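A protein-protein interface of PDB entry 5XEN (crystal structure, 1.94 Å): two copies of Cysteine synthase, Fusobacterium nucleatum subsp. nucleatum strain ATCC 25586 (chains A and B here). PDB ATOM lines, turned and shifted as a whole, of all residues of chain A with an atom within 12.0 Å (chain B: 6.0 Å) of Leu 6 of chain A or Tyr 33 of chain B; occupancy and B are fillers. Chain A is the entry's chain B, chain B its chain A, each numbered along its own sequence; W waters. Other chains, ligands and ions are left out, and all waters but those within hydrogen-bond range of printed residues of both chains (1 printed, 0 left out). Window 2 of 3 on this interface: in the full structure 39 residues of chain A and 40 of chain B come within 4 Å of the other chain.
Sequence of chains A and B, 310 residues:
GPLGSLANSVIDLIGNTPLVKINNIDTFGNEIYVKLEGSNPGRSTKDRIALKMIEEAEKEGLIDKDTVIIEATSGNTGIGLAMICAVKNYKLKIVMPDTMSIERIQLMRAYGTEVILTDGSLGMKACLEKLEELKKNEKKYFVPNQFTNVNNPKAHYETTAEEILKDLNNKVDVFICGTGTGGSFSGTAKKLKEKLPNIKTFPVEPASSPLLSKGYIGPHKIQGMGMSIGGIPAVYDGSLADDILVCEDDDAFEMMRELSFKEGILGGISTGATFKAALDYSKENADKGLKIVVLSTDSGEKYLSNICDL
Hydrophobic or aromatic side chains of chain A that line the printed part of chain B: Leu 6 and Ala 7. Among the printed residues, 10 pairs touch across the chains.
The backbone NH of Ala 7 of chain A sits at hydrogen-bond distance from the backbone carbonyl oxygen of Leu 19 of chain B, at 2.9 Å. N of Lys 21 of chain B is in hydrogen-bond range of O of Ala 7 of chain A, 3.0 Å away. O of Asn 8 of chain A lies close to O of Lys 21 of chain B (3.4 Å).
No position is printed for both chains. Of the 10 pairs that touch across the chains among the printed residues, none has its exchanged pair printed and touching as well.
Among the printed residues, merely in contact across the chains: Ala 7 of chain A with Val 20 of chain B (3.5 Å), Leu 6 of chain A with Leu 19 of chain B (3.5 Å), Leu 6 of chain A with Asp 167 of chain B (3.6 Å), Leu 6 of chain A with Leu 168 of chain B (3.6 Å), Ser 9 of chain A with Val 20 of chain B (3.7 Å), Leu 6 of chain A with Tyr 33 of chain B (3.9 Å) and Val 10 of chain A with Val 20 of chain B (3.98 Å).
N of Val 34 of chain B sits at hydrogen-bond distance from O of Val 20 of chain B (2.8 Å). NZ of Lys 21 of chain B is in salt-bridge range of OE2 of Glu 31 of chain B. The side-chain carboxylate (OE1) of Glu 31 of chain B is in hydrogen-bond range of the side-chain hydroxyl (OH) of Tyr 33 of chain B (3.0 Å). The backbone carbonyl oxygen (O) of Ile 292 of chain B sits at hydrogen-bond distance from the backbone NH (N) of Tyr 33 of chain B. The backbone NH (N) of Val 294 of chain B lies within hydrogen-bond range of the backbone carbonyl oxygen (O) of Tyr 33 of chain B, 2.9 Å away. The backbone NH (N) of Ser 9 of chain A is in hydrogen-bond range of the side-chain carboxylate (OD2) of Asp 12 of chain A, 3.2 Å away.
Water W1 lies within hydrogen-bond range of the side-chain carboxylate of Asp 167 of chain B (2.9 Å), the backbone NH of Leu 19 of chain B (3.0 Å) and the backbone NH of Leu 6 of chain A (3.4 Å).
Of chain B, only Leu 19 (3.5 Å), Tyr 33 (3.9 Å), Asp 167 (3.6 Å) and Leu 168 (3.6 Å) come within 4 Å of Leu 6 of chain A. Printed residues of chain B within 4 Å of Ala 7 of chain A: Leu 19 (2.9 Å), Val 20 (3.5 Å) and Lys 21 (3.0 Å). Printed residues of chain B within 4 Å of Asn 8 of chain A: Lys 21 (3.4 Å). Of the printed residues of chain B, Ser 9 of chain A touches Val 20. Printed residues of chain B within 4 Å of Val 10 of chain A: Val 20. Leu 13 of chain A touches none of the printed residues of chain B. Printed residues of chain A within 4 Å of Val 20 of chain B: Ala 7 (3.5 Å), Ser 9 (3.7 Å) and Val 10 (3.98 Å). Lys 21 of chain B touches two residues of chain A. No residue of chain A comes within 4 Å of Ile 22 of chain B. No residue of chain A comes within 4 Å of Glu 31 of chain B. No residue of chain A comes within 4 Å of Ile 32 of chain B. Of chain A, only Leu 6 comes within 4 Å of Tyr 33 of chain B. No residue of chain A comes within 4 Å of Val 34 of chain B. Of chain A, only Leu 6 comes within 4 Å of Leu 168 of chain B. No residue of chain A comes within 4 Å of Lys 291 of chain B. No residue of chain A comes within 4 Å of Val 293 of chain B. No residue of chain A comes within 4 Å of Val 294 of chain B. Leu 295 of chain B touches none of the printed residues of chain A.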
ATOM      1  N   LEU A   6      21.367 -12.649  -7.334  1.00  0.00           N
ATOM      2  CA  LEU A   6      22.729 -13.056  -6.872  1.00  0.00           C
ATOM      3  C   LEU A   6      23.687 -13.424  -8.005  1.00  0.00           C
ATOM      4  O   LEU A   6      23.296 -14.128  -8.931  1.00  0.00           O
ATOM      5  CB  LEU A   6      22.633 -14.295  -5.982  1.00  0.00           C
ATOM      6  CG  LEU A   6      21.655 -14.212  -4.835  1.00  0.00           C
ATOM      7  CD1 LEU A   6      21.703 -15.492  -4.017  1.00  0.00           C
ATOM      8  CD2 LEU A   6      21.979 -13.009  -3.961  1.00  0.00           C
ATOM      9  N   ALA A   7      24.951 -13.010  -7.866  1.00  0.00           N
ATOM     10  CA  ALA A   7      26.052 -13.526  -8.647  1.00  0.00           C
ATOM     11  C   ALA A   7      26.890 -14.454  -7.770  1.00  0.00           C
ATOM     12  O   ALA A   7      27.057 -14.208  -6.571  1.00  0.00           O
ATOM     13  CB  ALA A   7      26.915 -12.376  -9.131  1.00  0.00           C
ATOM     14  N   ASN A   8      27.459 -15.497  -8.345  1.00  0.00           N
ATOM     15  CA  ASN A   8      28.384 -16.328  -7.583  1.00  0.00           C
ATOM     16  C   ASN A   8      29.802 -15.799  -7.540  1.00  0.00           C
ATOM     17  O   ASN A   8      30.574 -16.142  -6.649  1.00  0.00           O
ATOM     18  CB  ASN A   8      28.385 -17.762  -8.086  1.00  0.00           C
ATOM     19  CG  ASN A   8      27.479 -18.630  -7.269  1.00  0.00           C
ATOM     20  OD1 ASN A   8      26.497 -19.149  -7.778  1.00  0.00           O
ATOM     21  ND2 ASN A   8      27.778 -18.741  -5.948  1.00  0.00           N
ATOM     22  N   SER A   9      30.163 -14.968  -8.518  1.00  0.00           N
ATOM     23  CA  SER A   9      31.416 -14.264  -8.470  1.00  0.00           C
ATOM     24  C   SER A   9      31.290 -13.064  -9.399  1.00  0.00           C
ATOM     25  O   SER A   9      30.286 -12.931 -10.124  1.00  0.00           O
ATOM     26  CB  SER A   9      32.562 -15.150  -8.944  1.00  0.00           C
ATOM     27  OG  SER A   9      32.571 -15.300 -10.357  1.00  0.00           O
ATOM     28  N   VAL A  10      32.303 -12.217  -9.396  1.00  0.00           N
ATOM     29  CA  VAL A  10      32.309 -11.069 -10.312  1.00  0.00           C
ATOM     30  C   VAL A  10      32.293 -11.508 -11.778  1.00  0.00           C
ATOM     31  O   VAL A  10      31.930 -10.706 -12.642  1.00  0.00           O
ATOM     32  CB  VAL A  10      33.510 -10.120 -10.060  1.00  0.00           C
ATOM     33  CG1 VAL A  10      33.383  -9.502  -8.672  1.00  0.00           C
ATOM     34  CG2 VAL A  10      34.820 -10.879 -10.174  1.00  0.00           C
ATOM     35  N   ILE A  11      32.704 -12.757 -12.064  1.00  0.00           N
ATOM     36  CA  ILE A  11      32.646 -13.294 -13.443  1.00  0.00           C
ATOM     37  C   ILE A  11      31.225 -13.215 -13.985  1.00  0.00           C
ATOM     38  O   ILE A  11      31.025 -12.893 -15.164  1.00  0.00           O
ATOM     39  CB  ILE A  11      33.178 -14.739 -13.559  1.00  0.00           C
ATOM     40  CG1 ILE A  11      34.688 -14.765 -13.345  1.00  0.00           C
ATOM     41  CG2 ILE A  11      32.754 -15.360 -14.886  1.00  0.00           C
ATOM     42  CD1 ILE A  11      35.275 -16.161 -13.236  1.00  0.00           C
ATOM     43  N   ASP A  12      30.237 -13.425 -13.109  1.00  0.00           N
ATOM     44  CA  ASP A  12      28.843 -13.344 -13.520  1.00  0.00           C
ATOM     45  C   ASP A  12      28.392 -11.917 -13.840  1.00  0.00           C
ATOM     46  O   ASP A  12      27.308 -11.716 -14.385  1.00  0.00           O
ATOM     47  CB  ASP A  12      27.897 -13.958 -12.476  1.00  0.00           C
ATOM     48  CG  ASP A  12      28.221 -15.409 -12.178  1.00  0.00           C
ATOM     49  OD1 ASP A  12      28.445 -16.168 -13.120  1.00  0.00           O
ATOM     50  OD2 ASP A  12      28.301 -15.786 -10.983  1.00  0.00           O
ATOM     51  N   LEU A  13      29.212 -10.920 -13.529  1.00  0.00           N
ATOM     52  CA  LEU A  13      28.857  -9.539 -13.821  1.00  0.00           C
ATOM     53  C   LEU A  13      29.400  -9.067 -15.171  1.00  0.00           C
ATOM     54  O   LEU A  13      29.146  -7.930 -15.587  1.00  0.00           O
ATOM     55  CB  LEU A  13      29.381  -8.626 -12.721  1.00  0.00           C
ATOM     56  CG  LEU A  13      28.995  -9.016 -11.274  1.00  0.00           C
ATOM     57  CD1 LEU A  13      29.564  -7.992 -10.276  1.00  0.00           C
ATOM     58  CD2 LEU A  13      27.486  -9.170 -11.123  1.00  0.00           C
ATOM     59  N   ILE A  14      30.184  -9.906 -15.840  1.00  0.00           N
ATOM     60  CA  ILE A  14      30.791  -9.522 -17.124  1.00  0.00           C
ATOM     61  C   ILE A  14      29.696  -9.457 -18.192  1.00  0.00           C
ATOM     62  O   ILE A  14      28.862 -10.328 -18.285  1.00  0.00           O
ATOM     63  CB  ILE A  14      31.903 -10.503 -17.528  1.00  0.00           C
ATOM     64  CG1 ILE A  14      33.075 -10.420 -16.536  1.00  0.00           C
ATOM     65  CG2 ILE A  14      32.385 -10.279 -18.964  1.00  0.00           C
ATOM     66  CD1 ILE A  14      34.136 -11.515 -16.685  1.00  0.00           C
ATOM     67  N   ASN A  16      26.480  -7.712 -20.534  1.00  0.00           N
ATOM     68  CA  ASN A  16      25.177  -7.073 -20.306  1.00  0.00           C
ATOM     69  C   ASN A  16      25.303  -5.613 -19.890  1.00  0.00           C
ATOM     70  O   ASN A  16      24.693  -5.154 -18.941  1.00  0.00           O
ATOM     71  CB  ASN A  16      24.343  -7.854 -19.291  1.00  0.00           C
ATOM     72  CG  ASN A  16      23.909  -9.200 -19.822  1.00  0.00           C
ATOM     73  OD1 ASN A  16      23.257  -9.278 -20.866  1.00  0.00           O
ATOM     74  ND2 ASN A  16      24.294 -10.272 -19.133  1.00  0.00           N
ATOM     75  N   LEU B  19      24.537  -8.277  -6.013  1.00  0.00           N
ATOM     76  CA  LEU B  19      24.905  -8.890  -4.737  1.00  0.00           C
ATOM     77  C   LEU B  19      25.775 -10.058  -5.153  1.00  0.00           C
ATOM     78  O   LEU B  19      25.346 -10.869  -5.966  1.00  0.00           O
ATOM     79  CB  LEU B  19      23.684  -9.516  -4.047  1.00  0.00           C
ATOM     80  CG  LEU B  19      23.080  -8.921  -2.821  1.00  0.00           C
ATOM     81  CD1 LEU B  19      22.141  -9.961  -2.184  1.00  0.00           C
ATOM     82  CD2 LEU B  19      24.128  -8.430  -1.828  1.00  0.00           C
ATOM     83  N   VAL B  20      26.992 -10.148  -4.642  1.00  0.00           N
ATOM     84  CA  VAL B  20      27.886 -11.215  -5.016  1.00  0.00           C
ATOM     85  C   VAL B  20      28.184 -12.057  -3.788  1.00  0.00           C
ATOM     86  O   VAL B  20      28.448 -11.513  -2.715  1.00  0.00           O
ATOM     87  CB  VAL B  20      29.197 -10.632  -5.564  1.00  0.00           C
ATOM     88  CG1 VAL B  20      30.091 -11.747  -6.115  1.00  0.00           C
ATOM     89  CG2 VAL B  20      28.851  -9.678  -6.700  1.00  0.00           C
ATOM     90  N   LYS B  21      28.155 -13.372  -3.939  1.00  0.00           N
ATOM     91  CA  LYS B  21      28.528 -14.276  -2.831  1.00  0.00           C
ATOM     92  C   LYS B  21      30.045 -14.381  -2.701  1.00  0.00           C
ATOM     93  O   LYS B  21      30.743 -14.421  -3.691  1.00  0.00           O
ATOM     94  CB  LYS B  21      27.940 -15.672  -3.043  1.00  0.00           C
ATOM     95  CG  LYS B  21      28.302 -16.641  -1.916  1.00  0.00           C
ATOM     96  CD  LYS B  21      27.384 -17.839  -1.929  1.00  0.00           C
ATOM     97  CE  LYS B  21      27.604 -18.708  -0.705  1.00  0.00           C
ATOM     98  NZ  LYS B  21      26.970 -20.044  -0.894  1.00  0.00           N
ATOM     99  N   ILE B  22      30.543 -14.427  -1.471  1.00  0.00           N
ATOM    100  CA  ILE B  22      31.949 -14.611  -1.202  1.00  0.00           C
ATOM    101  C   ILE B  22      32.243 -16.127  -1.179  1.00  0.00           C
ATOM    102  O   ILE B  22      31.658 -16.855  -0.375  1.00  0.00           O
ATOM    103  CB  ILE B  22      32.323 -13.993   0.149  1.00  0.00           C
ATOM    104  CG1 ILE B  22      32.104 -12.480   0.098  1.00  0.00           C
ATOM    105  CG2 ILE B  22      33.766 -14.271   0.521  1.00  0.00           C
ATOM    106  CD1 ILE B  22      33.081 -11.757  -0.796  1.00  0.00           C
ATOM    107  N   GLU B  31      27.029 -17.341   5.216  1.00  0.00           N
ATOM    108  CA  GLU B  31      27.176 -16.864   3.831  1.00  0.00           C
ATOM    109  C   GLU B  31      27.263 -15.339   3.872  1.00  0.00           C
ATOM    110  O   GLU B  31      26.444 -14.684   4.529  1.00  0.00           O
ATOM    111  CB  GLU B  31      26.005 -17.332   2.978  1.00  0.00           C
ATOM    112  CG  GLU B  31      25.865 -18.838   2.945  1.00  0.00           C
ATOM    113  CD  GLU B  31      24.756 -19.340   2.033  1.00  0.00           C
ATOM    114  OE1 GLU B  31      23.687 -18.699   1.970  1.00  0.00           O
ATOM    115  OE2 GLU B  31      24.954 -20.389   1.388  1.00  0.00           O
ATOM    116  N   ILE B  32      28.291 -14.782   3.234  1.00  0.00           N
ATOM    117  CA  ILE B  32      28.428 -13.344   3.141  1.00  0.00           C
ATOM    118  C   ILE B  32      28.225 -12.950   1.686  1.00  0.00           C
ATOM    119  O   ILE B  32      28.833 -13.540   0.777  1.00  0.00           O
ATOM    120  CB  ILE B  32      29.781 -12.830   3.662  1.00  0.00           C
ATOM    121  CG1 ILE B  32      29.994 -13.272   5.130  1.00  0.00           C
ATOM    122  CG2 ILE B  32      29.840 -11.303   3.553  1.00  0.00           C
ATOM    123  CD1 ILE B  32      31.238 -12.739   5.800  1.00  0.00           C
ATOM    124  N   TYR B  33      27.331 -11.987   1.488  1.00  0.00           N
ATOM    125  CA  TYR B  33      27.046 -11.416   0.184  1.00  0.00           C
ATOM    126  C   TYR B  33      27.449  -9.934   0.236  1.00  0.00           C
ATOM    127  O   TYR B  33      27.135  -9.227   1.203  1.00  0.00           O
ATOM    128  CB  TYR B  33      25.574 -11.504  -0.139  1.00  0.00           C
ATOM    129  CG  TYR B  33      25.049 -12.910  -0.214  1.00  0.00           C
ATOM    130  CD1 TYR B  33      25.081 -13.624  -1.413  1.00  0.00           C
ATOM    131  CD2 TYR B  33      24.515 -13.536   0.911  1.00  0.00           C
ATOM    132  CE1 TYR B  33      24.607 -14.929  -1.482  1.00  0.00           C
ATOM    133  CE2 TYR B  33      24.022 -14.831   0.845  1.00  0.00           C
ATOM    134  CZ  TYR B  33      24.088 -15.523  -0.345  1.00  0.00           C
ATOM    135  OH  TYR B  33      23.591 -16.821  -0.399  1.00  0.00           O
ATOM    136  N   VAL B  34      28.139  -9.488  -0.794  1.00  0.00           N
ATOM    137  CA  VAL B  34      28.573  -8.105  -0.854  1.00  0.00           C
ATOM    138  C   VAL B  34      27.735  -7.384  -1.898  1.00  0.00           C
ATOM    139  O   VAL B  34      27.640  -7.832  -3.051  1.00  0.00           O
ATOM    140  CB  VAL B  34      30.049  -8.008  -1.211  1.00  0.00           C
ATOM    141  CG1 VAL B  34      30.473  -6.555  -1.341  1.00  0.00           C
ATOM    142  CG2 VAL B  34      30.876  -8.731  -0.123  1.00  0.00           C
ATOM    143  N   LYS B  35      27.105  -6.291  -1.482  1.00  0.00           N
ATOM    144  CA  LYS B  35      26.320  -5.468  -2.403  1.00  0.00           C
ATOM    145  C   LYS B  35      27.275  -4.449  -3.010  1.00  0.00           C
ATOM    146  O   LYS B  35      27.804  -3.592  -2.313  1.00  0.00           O
ATOM    147  CB  LYS B  35      25.159  -4.798  -1.726  1.00  0.00           C
ATOM    148  CG  LYS B  35      24.251  -4.111  -2.752  1.00  0.00           C
ATOM    149  CD  LYS B  35      22.818  -4.036  -2.317  1.00  0.00           C
ATOM    150  CE  LYS B  35      21.911  -3.294  -3.284  1.00  0.00           C
ATOM    151  NZ  LYS B  35      21.638  -4.097  -4.526  1.00  0.00           N
ATOM    152  N   ASP B 167      16.684  -9.710  -4.006  1.00  0.00           N
ATOM    153  CA  ASP B 167      17.726 -10.617  -4.476  1.00  0.00           C
ATOM    154  C   ASP B 167      17.931 -11.825  -3.571  1.00  0.00           C
ATOM    155  O   ASP B 167      18.365 -12.877  -4.034  1.00  0.00           O
ATOM    156  CB  ASP B 167      19.055  -9.875  -4.671  1.00  0.00           C
ATOM    157  CG  ASP B 167      19.036  -8.944  -5.877  1.00  0.00           C
ATOM    158  OD1 ASP B 167      18.083  -9.020  -6.676  1.00  0.00           O
ATOM    159  OD2 ASP B 167      19.973  -8.118  -6.020  1.00  0.00           O
ATOM    160  N   LEU B 168      17.685 -11.670  -2.276  1.00  0.00           N
ATOM    161  CA  LEU B 168      17.837 -12.807  -1.354  1.00  0.00           C
ATOM    162  C   LEU B 168      16.494 -13.446  -0.997  1.00  0.00           C
ATOM    163  O   LEU B 168      16.436 -14.221  -0.064  1.00  0.00           O
ATOM    164  CB  LEU B 168      18.582 -12.369  -0.085  1.00  0.00           C
ATOM    165  CG  LEU B 168      20.079 -12.180  -0.247  1.00  0.00           C
ATOM    166  CD1 LEU B 168      20.703 -11.566   1.017  1.00  0.00           C
ATOM    167  CD2 LEU B 168      20.739 -13.501  -0.578  1.00  0.00           C
ATOM    168  N   LYS B 291      22.761 -15.493   6.758  1.00  0.00           N
ATOM    169  CA  LYS B 291      22.919 -14.780   5.493  1.00  0.00           C
ATOM    170  C   LYS B 291      23.266 -13.362   5.890  1.00  0.00           C
ATOM    171  O   LYS B 291      22.434 -12.640   6.461  1.00  0.00           O
ATOM    172  CB  LYS B 291      21.626 -14.828   4.706  1.00  0.00           C
ATOM    173  CG  LYS B 291      21.080 -16.243   4.454  1.00  0.00           C
ATOM    174  CD  LYS B 291      21.438 -16.727   3.044  1.00  0.00           C
ATOM    175  CE  LYS B 291      20.251 -17.245   2.251  1.00  0.00           C
ATOM    176  NZ  LYS B 291      19.418 -16.118   1.727  1.00  0.00           N
ATOM    177  N   ILE B 292      24.501 -12.979   5.605  1.00  0.00           N
ATOM    178  CA  ILE B 292      25.030 -11.685   6.037  1.00  0.00           C
ATOM    179  C   ILE B 292      25.225 -10.826   4.787  1.00  0.00           C
ATOM    180  O   ILE B 292      25.891 -11.269   3.842  1.00  0.00           O
ATOM    181  CB  ILE B 292      26.374 -11.855   6.772  1.00  0.00           C
ATOM    182  CG1 ILE B 292      26.189 -12.737   8.035  1.00  0.00           C
ATOM    183  CG2 ILE B 292      26.957 -10.483   7.152  1.00  0.00           C
ATOM    184  CD1 ILE B 292      27.487 -13.165   8.711  1.00  0.00           C
ATOM    185  N   VAL B 293      24.669  -9.624   4.791  1.00  0.00           N
ATOM    186  CA  VAL B 293      24.862  -8.700   3.650  1.00  0.00           C
ATOM    187  C   VAL B 293      25.724  -7.541   4.090  1.00  0.00           C
ATOM    188  O   VAL B 293      25.485  -6.942   5.152  1.00  0.00           O
ATOM    189  CB  VAL B 293      23.543  -8.171   3.093  1.00  0.00           C
ATOM    190  CG1 VAL B 293      23.782  -7.083   2.037  1.00  0.00           C
ATOM    191  CG2 VAL B 293      22.716  -9.325   2.513  1.00  0.00           C
ATOM    192  N   VAL B 294      26.772  -7.293   3.305  1.00  0.00           N
ATOM    193  CA  VAL B 294      27.694  -6.226   3.544  1.00  0.00           C
ATOM    194  C   VAL B 294      27.528  -5.228   2.403  1.00  0.00           C
ATOM    195  O   VAL B 294      27.589  -5.599   1.228  1.00  0.00           O
ATOM    196  CB  VAL B 294      29.132  -6.766   3.556  1.00  0.00           C
ATOM    197  CG1 VAL B 294      30.169  -5.650   3.463  1.00  0.00           C
ATOM    198  CG2 VAL B 294      29.316  -7.591   4.810  1.00  0.00           C
ATOM    199  N   LEU B 295      27.351  -3.964   2.746  1.00  0.00           N
ATOM    200  CA  LEU B 295      27.332  -2.932   1.733  1.00  0.00           C
ATOM    201  C   LEU B 295      28.754  -2.517   1.393  1.00  0.00           C
ATOM    202  O   LEU B 295      29.491  -2.072   2.268  1.00  0.00           O
ATOM    203  CB  LEU B 295      26.503  -1.742   2.203  1.00  0.00           C
ATOM    204  CG  LEU B 295      26.117  -0.781   1.079  1.00  0.00           C
ATOM    205  CD1 LEU B 295      24.903  -1.309   0.322  1.00  0.00           C
ATOM    206  CD2 LEU B 295      25.877   0.615   1.616  1.00  0.00           C
HETATM  207  O   HOH W   1      22.151  -9.380  -7.433  1.00  0.00           O
